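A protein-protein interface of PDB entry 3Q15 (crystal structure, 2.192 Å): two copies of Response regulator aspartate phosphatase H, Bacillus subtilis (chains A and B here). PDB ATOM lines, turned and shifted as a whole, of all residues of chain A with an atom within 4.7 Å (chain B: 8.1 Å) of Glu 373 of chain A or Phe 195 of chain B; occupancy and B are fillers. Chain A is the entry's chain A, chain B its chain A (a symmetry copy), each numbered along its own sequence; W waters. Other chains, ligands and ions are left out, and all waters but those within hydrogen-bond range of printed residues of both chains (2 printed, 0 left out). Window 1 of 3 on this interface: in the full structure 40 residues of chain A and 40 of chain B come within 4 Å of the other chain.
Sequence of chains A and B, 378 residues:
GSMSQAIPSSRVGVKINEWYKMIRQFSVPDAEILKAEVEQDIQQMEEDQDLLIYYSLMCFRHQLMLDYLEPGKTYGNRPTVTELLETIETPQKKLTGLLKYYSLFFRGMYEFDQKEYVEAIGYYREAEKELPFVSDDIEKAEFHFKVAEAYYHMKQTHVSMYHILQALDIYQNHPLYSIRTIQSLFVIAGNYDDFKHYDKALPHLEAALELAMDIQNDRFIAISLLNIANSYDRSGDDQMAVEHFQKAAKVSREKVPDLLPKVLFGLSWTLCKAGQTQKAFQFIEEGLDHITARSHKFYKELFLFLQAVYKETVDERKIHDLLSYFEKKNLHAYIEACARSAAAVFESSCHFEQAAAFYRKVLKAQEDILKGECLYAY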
ATOM      1  N   TYR A 117       2.434  23.586 -16.018  1.00  0.00           N
ATOM      2  CA  TYR A 117       1.060  24.064 -15.924  1.00  0.00           C
ATOM      3  C   TYR A 117       0.209  23.299 -14.915  1.00  0.00           C
ATOM      4  O   TYR A 117      -0.565  23.898 -14.167  1.00  0.00           O
ATOM      5  CB  TYR A 117       0.395  24.063 -17.303  1.00  0.00           C
ATOM      6  CG  TYR A 117       0.999  25.067 -18.260  1.00  0.00           C
ATOM      7  CD1 TYR A 117       1.529  26.263 -17.797  1.00  0.00           C
ATOM      8  CD2 TYR A 117       1.051  24.812 -19.623  1.00  0.00           C
ATOM      9  CE1 TYR A 117       2.081  27.182 -18.659  1.00  0.00           C
ATOM     10  CE2 TYR A 117       1.607  25.725 -20.499  1.00  0.00           C
ATOM     11  CZ  TYR A 117       2.118  26.907 -20.013  1.00  0.00           C
ATOM     12  OH  TYR A 117       2.669  27.816 -20.883  1.00  0.00           O
ATOM     13  N   LYS A 155      -3.991  28.358 -22.741  1.00  0.00           N
ATOM     14  CA  LYS A 155      -5.008  27.919 -23.688  1.00  0.00           C
ATOM     15  C   LYS A 155      -6.114  27.107 -23.017  1.00  0.00           C
ATOM     16  O   LYS A 155      -6.752  26.271 -23.654  1.00  0.00           O
ATOM     17  CB  LYS A 155      -4.387  27.125 -24.844  1.00  0.00           C
ATOM     18  CG  LYS A 155      -3.697  27.987 -25.888  1.00  0.00           C
ATOM     19  CD  LYS A 155      -2.219  27.650 -25.993  1.00  0.00           C
ATOM     20  CE  LYS A 155      -1.566  28.364 -27.167  1.00  0.00           C
ATOM     21  NZ  LYS A 155      -0.138  27.971 -27.339  1.00  0.00           N
ATOM     22  N   ILE A 369       3.381  23.766 -31.886  1.00  0.00           N
ATOM     23  CA  ILE A 369       2.829  24.628 -30.849  1.00  0.00           C
ATOM     24  C   ILE A 369       2.262  23.784 -29.713  1.00  0.00           C
ATOM     25  O   ILE A 369       2.606  23.983 -28.546  1.00  0.00           O
ATOM     26  CB  ILE A 369       1.729  25.551 -31.416  1.00  0.00           C
ATOM     27  CG1 ILE A 369       2.328  26.527 -32.427  1.00  0.00           C
ATOM     28  CG2 ILE A 369       1.033  26.324 -30.295  1.00  0.00           C
ATOM     29  CD1 ILE A 369       1.311  27.476 -33.028  1.00  0.00           C
ATOM     30  N   LEU A 370       1.401  22.835 -30.063  1.00  0.00           N
ATOM     31  CA  LEU A 370       0.803  21.943 -29.077  1.00  0.00           C
ATOM     32  C   LEU A 370       1.850  21.215 -28.237  1.00  0.00           C
ATOM     33  O   LEU A 370       1.713  21.129 -27.021  1.00  0.00           O
ATOM     34  CB  LEU A 370      -0.118  20.933 -29.762  1.00  0.00           C
ATOM     35  CG  LEU A 370      -1.492  21.486 -30.152  1.00  0.00           C
ATOM     36  CD1 LEU A 370      -2.256  20.502 -31.021  1.00  0.00           C
ATOM     37  CD2 LEU A 370      -2.290  21.849 -28.904  1.00  0.00           C
ATOM     38  N   LYS A 371       2.896  20.695 -28.881  1.00  0.00           N
ATOM     39  CA  LYS A 371       3.937  19.966 -28.159  1.00  0.00           C
ATOM     40  C   LYS A 371       4.650  20.863 -27.150  1.00  0.00           C
ATOM     41  O   LYS A 371       5.015  20.428 -26.057  1.00  0.00           O
ATOM     42  CB  LYS A 371       4.954  19.344 -29.126  1.00  0.00           C
ATOM     43  CG  LYS A 371       4.400  18.229 -29.993  1.00  0.00           C
ATOM     44  CD  LYS A 371       5.527  17.466 -30.666  1.00  0.00           C
ATOM     45  CE  LYS A 371       5.028  16.201 -31.345  1.00  0.00           C
ATOM     46  NZ  LYS A 371       6.146  15.422 -31.953  1.00  0.00           N
ATOM     47  N   GLY A 372       4.850  22.121 -27.523  1.00  0.00           N
ATOM     48  CA  GLY A 372       5.512  23.064 -26.643  1.00  0.00           C
ATOM     49  C   GLY A 372       4.666  23.468 -25.451  1.00  0.00           C
ATOM     50  O   GLY A 372       5.170  24.075 -24.508  1.00  0.00           O
ATOM     51  N   GLU A 373       3.378  23.134 -25.493  1.00  0.00           N
ATOM     52  CA  GLU A 373       2.452  23.492 -24.420  1.00  0.00           C
ATOM     53  C   GLU A 373       2.477  22.460 -23.296  1.00  0.00           C
ATOM     54  O   GLU A 373       1.992  22.721 -22.199  1.00  0.00           O
ATOM     55  CB  GLU A 373       1.019  23.616 -24.956  1.00  0.00           C
ATOM     56  CG  GLU A 373       0.815  24.655 -26.050  1.00  0.00           C
ATOM     57  CD  GLU A 373      -0.639  24.727 -26.531  1.00  0.00           C
ATOM     58  OE1 GLU A 373      -0.885  25.320 -27.604  1.00  0.00           O
ATOM     59  OE2 GLU A 373      -1.538  24.195 -25.837  1.00  0.00           O
ATOM     60  N   CYS A 374       3.033  21.286 -23.576  1.00  0.00           N
ATOM     61  CA  CYS A 374       3.062  20.202 -22.601  1.00  0.00           C
ATOM     62  C   CYS A 374       4.485  19.700 -22.393  1.00  0.00           C
ATOM     63  O   CYS A 374       4.991  18.892 -23.178  1.00  0.00           O
ATOM     64  CB  CYS A 374       2.169  19.057 -23.068  1.00  0.00           C
ATOM     65  SG  CYS A 374       2.114  17.633 -21.963  1.00  0.00           S
ATOM     66  N   LEU A 375       5.129  20.178 -21.332  1.00  0.00           N
ATOM     67  CA  LEU A 375       6.518  19.827 -21.074  1.00  0.00           C
ATOM     68  C   LEU A 375       6.670  18.863 -19.903  1.00  0.00           C
ATOM     69  O   LEU A 375       7.744  18.304 -19.698  1.00  0.00           O
ATOM     70  CB  LEU A 375       7.358  21.083 -20.834  1.00  0.00           C
ATOM     71  CG  LEU A 375       7.365  22.098 -21.979  1.00  0.00           C
ATOM     72  CD1 LEU A 375       8.208  23.313 -21.617  1.00  0.00           C
ATOM     73  CD2 LEU A 375       7.862  21.456 -23.268  1.00  0.00           C
ATOM     74  N   TYR A 376       5.602  18.663 -19.137  1.00  0.00           N
ATOM     75  CA  TYR A 376       5.668  17.745 -17.999  1.00  0.00           C
ATOM     76  C   TYR A 376       5.615  16.288 -18.448  1.00  0.00           C
ATOM     77  O   TYR A 376       5.386  15.997 -19.627  1.00  0.00           O
ATOM     78  CB  TYR A 376       4.562  18.039 -16.986  1.00  0.00           C
ATOM     79  CG  TYR A 376       3.183  18.198 -17.588  1.00  0.00           C
ATOM     80  CD1 TYR A 376       2.421  17.091 -17.940  1.00  0.00           C
ATOM     81  CD2 TYR A 376       2.635  19.460 -17.783  1.00  0.00           C
ATOM     82  CE1 TYR A 376       1.152  17.238 -18.482  1.00  0.00           C
ATOM     83  CE2 TYR A 376       1.371  19.618 -18.325  1.00  0.00           C
ATOM     84  CZ  TYR A 376       0.632  18.505 -18.670  1.00  0.00           C
ATOM     85  OH  TYR A 376      -0.626  18.664 -19.206  1.00  0.00           O
ATOM     86  N   LYS B 155     -11.779  20.076 -23.751  1.00  0.00           N
ATOM     87  CA  LYS B 155     -10.458  20.409 -24.269  1.00  0.00           C
ATOM     88  C   LYS B 155      -9.685  21.338 -23.336  1.00  0.00           C
ATOM     89  O   LYS B 155      -8.823  22.095 -23.778  1.00  0.00           O
ATOM     90  CB  LYS B 155     -10.547  21.016 -25.676  1.00  0.00           C
ATOM     91  CG  LYS B 155     -10.792  19.996 -26.776  1.00  0.00           C
ATOM     92  CD  LYS B 155     -12.098  20.272 -27.503  1.00  0.00           C
ATOM     93  CE  LYS B 155     -12.252  19.382 -28.728  1.00  0.00           C
ATOM     94  NZ  LYS B 155     -13.484  19.707 -29.504  1.00  0.00           N
ATOM     95  N   GLN B 156     -10.004  21.281 -22.048  1.00  0.00           N
ATOM     96  CA  GLN B 156      -9.202  21.952 -21.035  1.00  0.00           C
ATOM     97  C   GLN B 156      -8.287  20.877 -20.468  1.00  0.00           C
ATOM     98  O   GLN B 156      -8.460  20.414 -19.340  1.00  0.00           O
ATOM     99  CB  GLN B 156     -10.088  22.557 -19.944  1.00  0.00           C
ATOM    100  CG  GLN B 156     -11.267  23.388 -20.462  1.00  0.00           C
ATOM    101  CD  GLN B 156     -10.829  24.589 -21.279  1.00  0.00           C
ATOM    102  OE1 GLN B 156     -10.652  24.495 -22.491  1.00  0.00           O
ATOM    103  NE2 GLN B 156     -10.646  25.724 -20.616  1.00  0.00           N
ATOM    104  N   THR B 157      -7.319  20.481 -21.283  1.00  0.00           N
ATOM    105  CA  THR B 157      -6.530  19.279 -21.051  1.00  0.00           C
ATOM    106  C   THR B 157      -5.588  19.378 -19.850  1.00  0.00           C
ATOM    107  O   THR B 157      -5.343  18.380 -19.175  1.00  0.00           O
ATOM    108  CB  THR B 157      -5.740  18.895 -22.325  1.00  0.00           C
ATOM    109  OG1 THR B 157      -6.624  18.900 -23.456  1.00  0.00           O
ATOM    110  CG2 THR B 157      -5.102  17.510 -22.178  1.00  0.00           C
ATOM    111  N   HIS B 158      -5.059  20.571 -19.583  1.00  0.00           N
ATOM    112  CA  HIS B 158      -4.194  20.773 -18.417  1.00  0.00           C
ATOM    113  C   HIS B 158      -4.980  20.603 -17.125  1.00  0.00           C
ATOM    114  O   HIS B 158      -4.520  19.960 -16.177  1.00  0.00           O
ATOM    115  CB  HIS B 158      -3.553  22.159 -18.437  1.00  0.00           C
ATOM    116  CG  HIS B 158      -2.490  22.316 -19.475  1.00  0.00           C
ATOM    117  ND1 HIS B 158      -1.478  21.397 -19.646  1.00  0.00           N
ATOM    118  CD2 HIS B 158      -2.276  23.285 -20.398  1.00  0.00           C
ATOM    119  CE1 HIS B 158      -0.688  21.790 -20.629  1.00  0.00           C
ATOM    120  NE2 HIS B 158      -1.151  22.933 -21.102  1.00  0.00           N
ATOM    121  N   VAL B 159      -6.167  21.197 -17.093  1.00  0.00           N
ATOM    122  CA  VAL B 159      -7.039  21.108 -15.932  1.00  0.00           C
ATOM    123  C   VAL B 159      -7.521  19.676 -15.766  1.00  0.00           C
ATOM    124  O   VAL B 159      -7.656  19.184 -14.650  1.00  0.00           O
ATOM    125  CB  VAL B 159      -8.252  22.049 -16.069  1.00  0.00           C
ATOM    126  CG1 VAL B 159      -9.173  21.909 -14.863  1.00  0.00           C
ATOM    127  CG2 VAL B 159      -7.779  23.485 -16.221  1.00  0.00           C
ATOM    128  N   SER B 160      -7.770  19.009 -16.886  1.00  0.00           N
ATOM    129  CA  SER B 160      -8.168  17.611 -16.858  1.00  0.00           C
ATOM    130  C   SER B 160      -7.083  16.772 -16.198  1.00  0.00           C
ATOM    131  O   SER B 160      -7.368  15.918 -15.358  1.00  0.00           O
ATOM    132  CB  SER B 160      -8.419  17.106 -18.277  1.00  0.00           C
ATOM    133  OG  SER B 160      -8.810  15.743 -18.271  1.00  0.00           O
ATOM    134  N   MET B 161      -5.836  17.020 -16.591  1.00  0.00           N
ATOM    135  CA  MET B 161      -4.703  16.282 -16.056  1.00  0.00           C
ATOM    136  C   MET B 161      -4.575  16.519 -14.554  1.00  0.00           C
ATOM    137  O   MET B 161      -4.356  15.586 -13.783  1.00  0.00           O
ATOM    138  CB  MET B 161      -3.407  16.681 -16.766  1.00  0.00           C
ATOM    139  CG  MET B 161      -2.247  15.743 -16.465  1.00  0.00           C
ATOM    140  SD  MET B 161      -2.450  14.137 -17.259  1.00  0.00           S
ATOM    141  CE  MET B 161      -1.816  14.476 -18.897  1.00  0.00           C
ATOM    142  N   ILE B 188      -5.307   9.772 -18.720  1.00  0.00           N
ATOM    143  CA  ILE B 188      -3.996  10.409 -18.735  1.00  0.00           C
ATOM    144  C   ILE B 188      -3.351  10.310 -20.118  1.00  0.00           C
ATOM    145  O   ILE B 188      -2.821  11.293 -20.639  1.00  0.00           O
ATOM    146  CB  ILE B 188      -3.068   9.789 -17.680  1.00  0.00           C
ATOM    147  CG1 ILE B 188      -3.647   9.999 -16.281  1.00  0.00           C
ATOM    148  CG2 ILE B 188      -1.675  10.387 -17.772  1.00  0.00           C
ATOM    149  CD1 ILE B 188      -2.873   9.273 -15.182  1.00  0.00           C
ATOM    150  N   ALA B 189      -3.397   9.119 -20.708  1.00  0.00           N
ATOM    151  CA  ALA B 189      -2.879   8.920 -22.056  1.00  0.00           C
ATOM    152  C   ALA B 189      -3.614   9.808 -23.055  1.00  0.00           C
ATOM    153  O   ALA B 189      -2.990  10.483 -23.872  1.00  0.00           O
ATOM    154  CB  ALA B 189      -3.001   7.463 -22.458  1.00  0.00           C
ATOM    155  N   GLY B 190      -4.944   9.799 -22.983  1.00  0.00           N
ATOM    156  CA  GLY B 190      -5.765  10.598 -23.874  1.00  0.00           C
ATOM    157  C   GLY B 190      -5.392  12.065 -23.805  1.00  0.00           C
ATOM    158  O   GLY B 190      -5.344  12.754 -24.827  1.00  0.00           O
ATOM    159  N   ASN B 191      -5.115  12.542 -22.595  1.00  0.00           N
ATOM    160  CA  ASN B 191      -4.721  13.931 -22.390  1.00  0.00           C
ATOM    161  C   ASN B 191      -3.398  14.259 -23.071  1.00  0.00           C
ATOM    162  O   ASN B 191      -3.265  15.285 -23.744  1.00  0.00           O
ATOM    163  CB  ASN B 191      -4.659  14.267 -20.896  1.00  0.00           C
ATOM    164  CG  ASN B 191      -6.038  14.402 -20.274  1.00  0.00           C
ATOM    165  OD1 ASN B 191      -7.040  14.520 -20.983  1.00  0.00           O
ATOM    166  ND2 ASN B 191      -6.096  14.391 -18.947  1.00  0.00           N
ATOM    167  N   TYR B 192      -2.417  13.382 -22.893  1.00  0.00           N
ATOM    168  CA  TYR B 192      -1.141  13.536 -23.575  1.00  0.00           C
ATOM    169  C   TYR B 192      -1.324  13.570 -25.084  1.00  0.00           C
ATOM    170  O   TYR B 192      -0.667  14.346 -25.772  1.00  0.00           O
ATOM    171  CB  TYR B 192      -0.173  12.423 -23.182  1.00  0.00           C
ATOM    172  CG  TYR B 192       0.548  12.690 -21.885  1.00  0.00           C
ATOM    173  CD1 TYR B 192       1.327  13.829 -21.731  1.00  0.00           C
ATOM    174  CD2 TYR B 192       0.465  11.802 -20.821  1.00  0.00           C
ATOM    175  CE1 TYR B 192       1.997  14.081 -20.556  1.00  0.00           C
ATOM    176  CE2 TYR B 192       1.134  12.046 -19.636  1.00  0.00           C
ATOM    177  CZ  TYR B 192       1.899  13.188 -19.510  1.00  0.00           C
ATOM    178  OH  TYR B 192       2.569  13.451 -18.339  1.00  0.00           O
ATOM    179  N   ASP B 193      -2.220  12.724 -25.586  1.00  0.00           N
ATOM    180  CA  ASP B 193      -2.526  12.682 -27.010  1.00  0.00           C
ATOM    181  C   ASP B 193      -2.957  14.056 -27.530  1.00  0.00           C
ATOM    182  O   ASP B 193      -2.601  14.435 -28.645  1.00  0.00           O
ATOM    183  CB  ASP B 193      -3.605  11.637 -27.306  1.00  0.00           C
ATOM    184  CG  ASP B 193      -3.097  10.211 -27.167  1.00  0.00           C
ATOM    185  OD1 ASP B 193      -1.866  10.011 -27.072  1.00  0.00           O
ATOM    186  OD2 ASP B 193      -3.933   9.285 -27.168  1.00  0.00           O
ATOM    187  N   ASP B 194      -3.702  14.801 -26.713  1.00  0.00           N
ATOM    188  CA  ASP B 194      -4.158  16.139 -27.094  1.00  0.00           C
ATOM    189  C   ASP B 194      -2.996  17.068 -27.431  1.00  0.00           C
ATOM    190  O   ASP B 194      -3.146  17.999 -28.219  1.00  0.00           O
ATOM    191  CB  ASP B 194      -5.017  16.767 -25.991  1.00  0.00           C
ATOM    192  CG  ASP B 194      -6.459  16.298 -26.030  1.00  0.00           C
ATOM    193  OD1 ASP B 194      -6.857  15.655 -27.022  1.00  0.00           O
ATOM    194  OD2 ASP B 194      -7.198  16.589 -25.066  1.00  0.00           O
ATOM    195  N   PHE B 195      -1.839  16.814 -26.830  1.00  0.00           N
ATOM    196  CA  PHE B 195      -0.658  17.626 -27.099  1.00  0.00           C
ATOM    197  C   PHE B 195       0.287  16.915 -28.059  1.00  0.00           C
ATOM    198  O   PHE B 195       1.435  17.328 -28.236  1.00  0.00           O
ATOM    199  CB  PHE B 195       0.071  17.964 -25.798  1.00  0.00           C
ATOM    200  CG  PHE B 195      -0.766  18.732 -24.818  1.00  0.00           C
ATOM    201  CD1 PHE B 195      -1.005  20.084 -25.004  1.00  0.00           C
ATOM    202  CD2 PHE B 195      -1.315  18.104 -23.712  1.00  0.00           C
ATOM    203  CE1 PHE B 195      -1.779  20.800 -24.104  1.00  0.00           C
ATOM    204  CE2 PHE B 195      -2.087  18.813 -22.814  1.00  0.00           C
ATOM    205  CZ  PHE B 195      -2.321  20.162 -23.011  1.00  0.00           C
ATOM    206  N   LYS B 196      -0.208  15.843 -28.672  1.00  0.00           N
ATOM    207  CA  LYS B 196       0.567  15.051 -29.631  1.00  0.00           C
ATOM    208  C   LYS B 196       1.792  14.404 -28.992  1.00  0.00           C
ATOM    209  O   LYS B 196       2.768  14.110 -29.677  1.00  0.00           O
ATOM    210  CB  LYS B 196       1.009  15.908 -30.821  1.00  0.00           C
ATOM    211  CG  LYS B 196      -0.088  16.770 -31.424  1.00  0.00           C
ATOM    212  CD  LYS B 196      -1.247  15.931 -31.921  1.00  0.00           C
ATOM    213  CE  LYS B 196      -2.310  16.816 -32.552  1.00  0.00           C
ATOM    214  NZ  LYS B 196      -3.471  16.035 -33.052  1.00  0.00           N
ATOM    215  N   HIS B 197       1.745  14.188 -27.681  1.00  0.00           N
ATOM    216  CA  HIS B 197       2.844  13.521 -26.997  1.00  0.00           C
ATOM    217  C   HIS B 197       2.533  12.050 -26.773  1.00  0.00           C
ATOM    218  O   HIS B 197       2.419  11.588 -25.638  1.00  0.00           O
ATOM    219  CB  HIS B 197       3.158  14.210 -25.673  1.00  0.00           C
ATOM    220  CG  HIS B 197       4.080  15.379 -25.810  1.00  0.00           C
ATOM    221  ND1 HIS B 197       3.666  16.679 -25.627  1.00  0.00           N
ATOM    222  CD2 HIS B 197       5.397  15.442 -26.115  1.00  0.00           C
ATOM    223  CE1 HIS B 197       4.690  17.495 -25.811  1.00  0.00           C
ATOM    224  NE2 HIS B 197       5.752  16.769 -26.107  1.00  0.00           N
ATOM    225  N   TYR B 198       2.395  11.318 -27.870  1.00  0.00           N
ATOM    226  CA  TYR B 198       2.059   9.904 -27.809  1.00  0.00           C
ATOM    227  C   TYR B 198       3.100   9.115 -27.019  1.00  0.00           C
ATOM    228  O   TYR B 198       2.768   8.147 -26.336  1.00  0.00           O
ATOM    229  CB  TYR B 198       1.916   9.340 -29.223  1.00  0.00           C
ATOM    230  CG  TYR B 198       1.141  10.252 -30.146  1.00  0.00           C
ATOM    231  CD1 TYR B 198      -0.233  10.404 -30.012  1.00  0.00           C
ATOM    232  CD2 TYR B 198       1.785  10.969 -31.151  1.00  0.00           C
ATOM    233  CE1 TYR B 198      -0.947  11.242 -30.855  1.00  0.00           C
ATOM    234  CE2 TYR B 198       1.078  11.810 -31.999  1.00  0.00           C
ATOM    235  CZ  TYR B 198      -0.284  11.941 -31.845  1.00  0.00           C
ATOM    236  OH  TYR B 198      -0.991  12.773 -32.681  1.00  0.00           O
ATOM    237  N   ASP B 199       4.357   9.533 -27.106  1.00  0.00           N
ATOM    238  CA  ASP B 199       5.419   8.866 -26.366  1.00  0.00           C
ATOM    239  C   ASP B 199       5.209   8.987 -24.852  1.00  0.00           C
ATOM    240  O   ASP B 199       5.595   8.099 -24.097  1.00  0.00           O
ATOM    241  CB  ASP B 199       6.795   9.400 -26.778  1.00  0.00           C
ATOM    242  CG  ASP B 199       6.926  10.898 -26.582  1.00  0.00           C
ATOM    243  OD1 ASP B 199       7.995  11.347 -26.113  1.00  0.00           O
ATOM    244  OD2 ASP B 199       5.965  11.631 -26.899  1.00  0.00           O
ATOM    245  N   LYS B 200       4.587  10.076 -24.412  1.00  0.00           N
ATOM    246  CA  LYS B 200       4.299  10.246 -22.990  1.00  0.00           C
ATOM    247  C   LYS B 200       3.096   9.414 -22.573  1.00  0.00           C
ATOM    248  O   LYS B 200       3.016   8.953 -21.437  1.00  0.00           O
ATOM    249  CB  LYS B 200       4.078  11.719 -22.648  1.00  0.00           C
ATOM    250  CG  LYS B 200       5.344  12.550 -22.711  1.00  0.00           C
ATOM    251  CD  LYS B 200       5.047  14.022 -22.496  1.00  0.00           C
ATOM    252  CE  LYS B 200       6.306  14.863 -22.634  1.00  0.00           C
ATOM    253  NZ  LYS B 200       6.002  16.306 -22.449  1.00  0.00           N
HETATM  254  O   HOH W   1      -1.420  24.876 -23.063  1.00  0.00           O
HETATM  255  O   HOH W   2       3.861  13.545 -32.042  1.00  0.00           O
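Tyr 117 of chain A touches His 158 of chain B. Leu 370 of chain A touches Asp 194 of chain B (CD1 to O, 3.9 Å). Lys 371 of chain A touches Phe 195 of chain B (CG to O, 3.6 Å). Lys 196 of chain B touches Lys 371 of chain A (O to CE, 3.5 Å). Lys 371 of chain A touches His 197 of chain B. Cys 374 of chain A touches Phe 195 of chain B. His 197 of chain B touches Cys 374 of chain A (CE1 to O, 3.0 Å). C of Leu 375 of chain A touches NZ of Lys 200 of chain B, 3.7 Å away. Tyr 192 of chain B touches Tyr 376 of chain A (OH to CD1, 3.7 Å). CE2 of Phe 195 of chain B touches OH of Tyr 376 of chain A, at 3.9 Å.
Position printed for both chains: 155. Of the 18 pairs that touch across the chains among the printed residues, none has its exchanged pair printed and touching as well.
Lys 155 of chain A touches none of the printed residues of chain B. Of the printed residues of chain B, Cys 374 of chain A touches Tyr 192 (3.8 Å), Phe 195 (3.4 Å), His 197 (3.0 Å) and Lys 200 (2.9 Å). Printed residues of chain B within 4 Å of Leu 375 of chain A: Lys 200. Of the printed residues of chain B, Tyr 376 of chain A touches His 158 (2.9 Å), Tyr 192 (3.7 Å), Phe 195 (3.9 Å) and Lys 200 (2.9 Å). Phe 195 of chain B touches just these residues of chain A: Leu 370, Lys 371, Glu 373, Cys 374 and Tyr 376. The nearest residue of chain B that does not touch Glu 373 of chain A is His 197 of chain B (5.8 Å). The nearest printed residue of chain A that does not touch His 158 of chain B is Cys 374 of chain A (4.5 Å).
Printed residues of chain B that touch a printed residue of chain A: His 158, Tyr 192, Asp 194, Phe 195, Lys 196, His 197 and Lys 200. Along chain B the printed residues that touch a printed residue of chain A span positions 158 to 200. Hydrophobic or aromatic side chains of chain A that line the printed part of chain B: Tyr 117, Leu 370 and Tyr 376.
The side-chain amino group (NZ) of Lys 155 of chain A is in salt-bridge range of the side-chain carboxylate (OE1) of Glu 373 of chain A (2.8 Å). ND1 of His 197 of chain B is in hydrogen-bond range of O of Phe 195 of chain B (3.5 Å). The backbone NH of His 197 of chain B lies within hydrogen-bond range of the backbone carbonyl oxygen of Tyr 192 of chain B (3.1 Å). OG1 of Thr 157 of chain B lies within hydrogen-bond range of OD2 of Asp 194 of chain B (2.9 Å).
The side-chain hydroxyl of Tyr 376 of chain A is in hydrogen-bond range of a ring nitrogen (ND1) of His 158 of chain B (2.9 Å). The backbone carbonyl oxygen (O) of Tyr 376 of chain A lies within hydrogen-bond range of the side-chain amino group (NZ) of Lys 200 of chain B (2.9 Å). O of Glu 373 of chain A lies close to NE2 of His 158 of chain B, at 3.3 Å. NZ of Lys 200 of chain B is in hydrogen-bond range of O of Cys 374 of chain A (2.9 Å).
Water W2 lies within hydrogen-bond range of O of Lys 196 of chain B and NZ of Lys 371 of chain A. Water W1 lies within hydrogen-bond range of NE2 of His 158 of chain B (2.8 Å) and OE2 of Glu 373 of chain A (2.9 Å).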
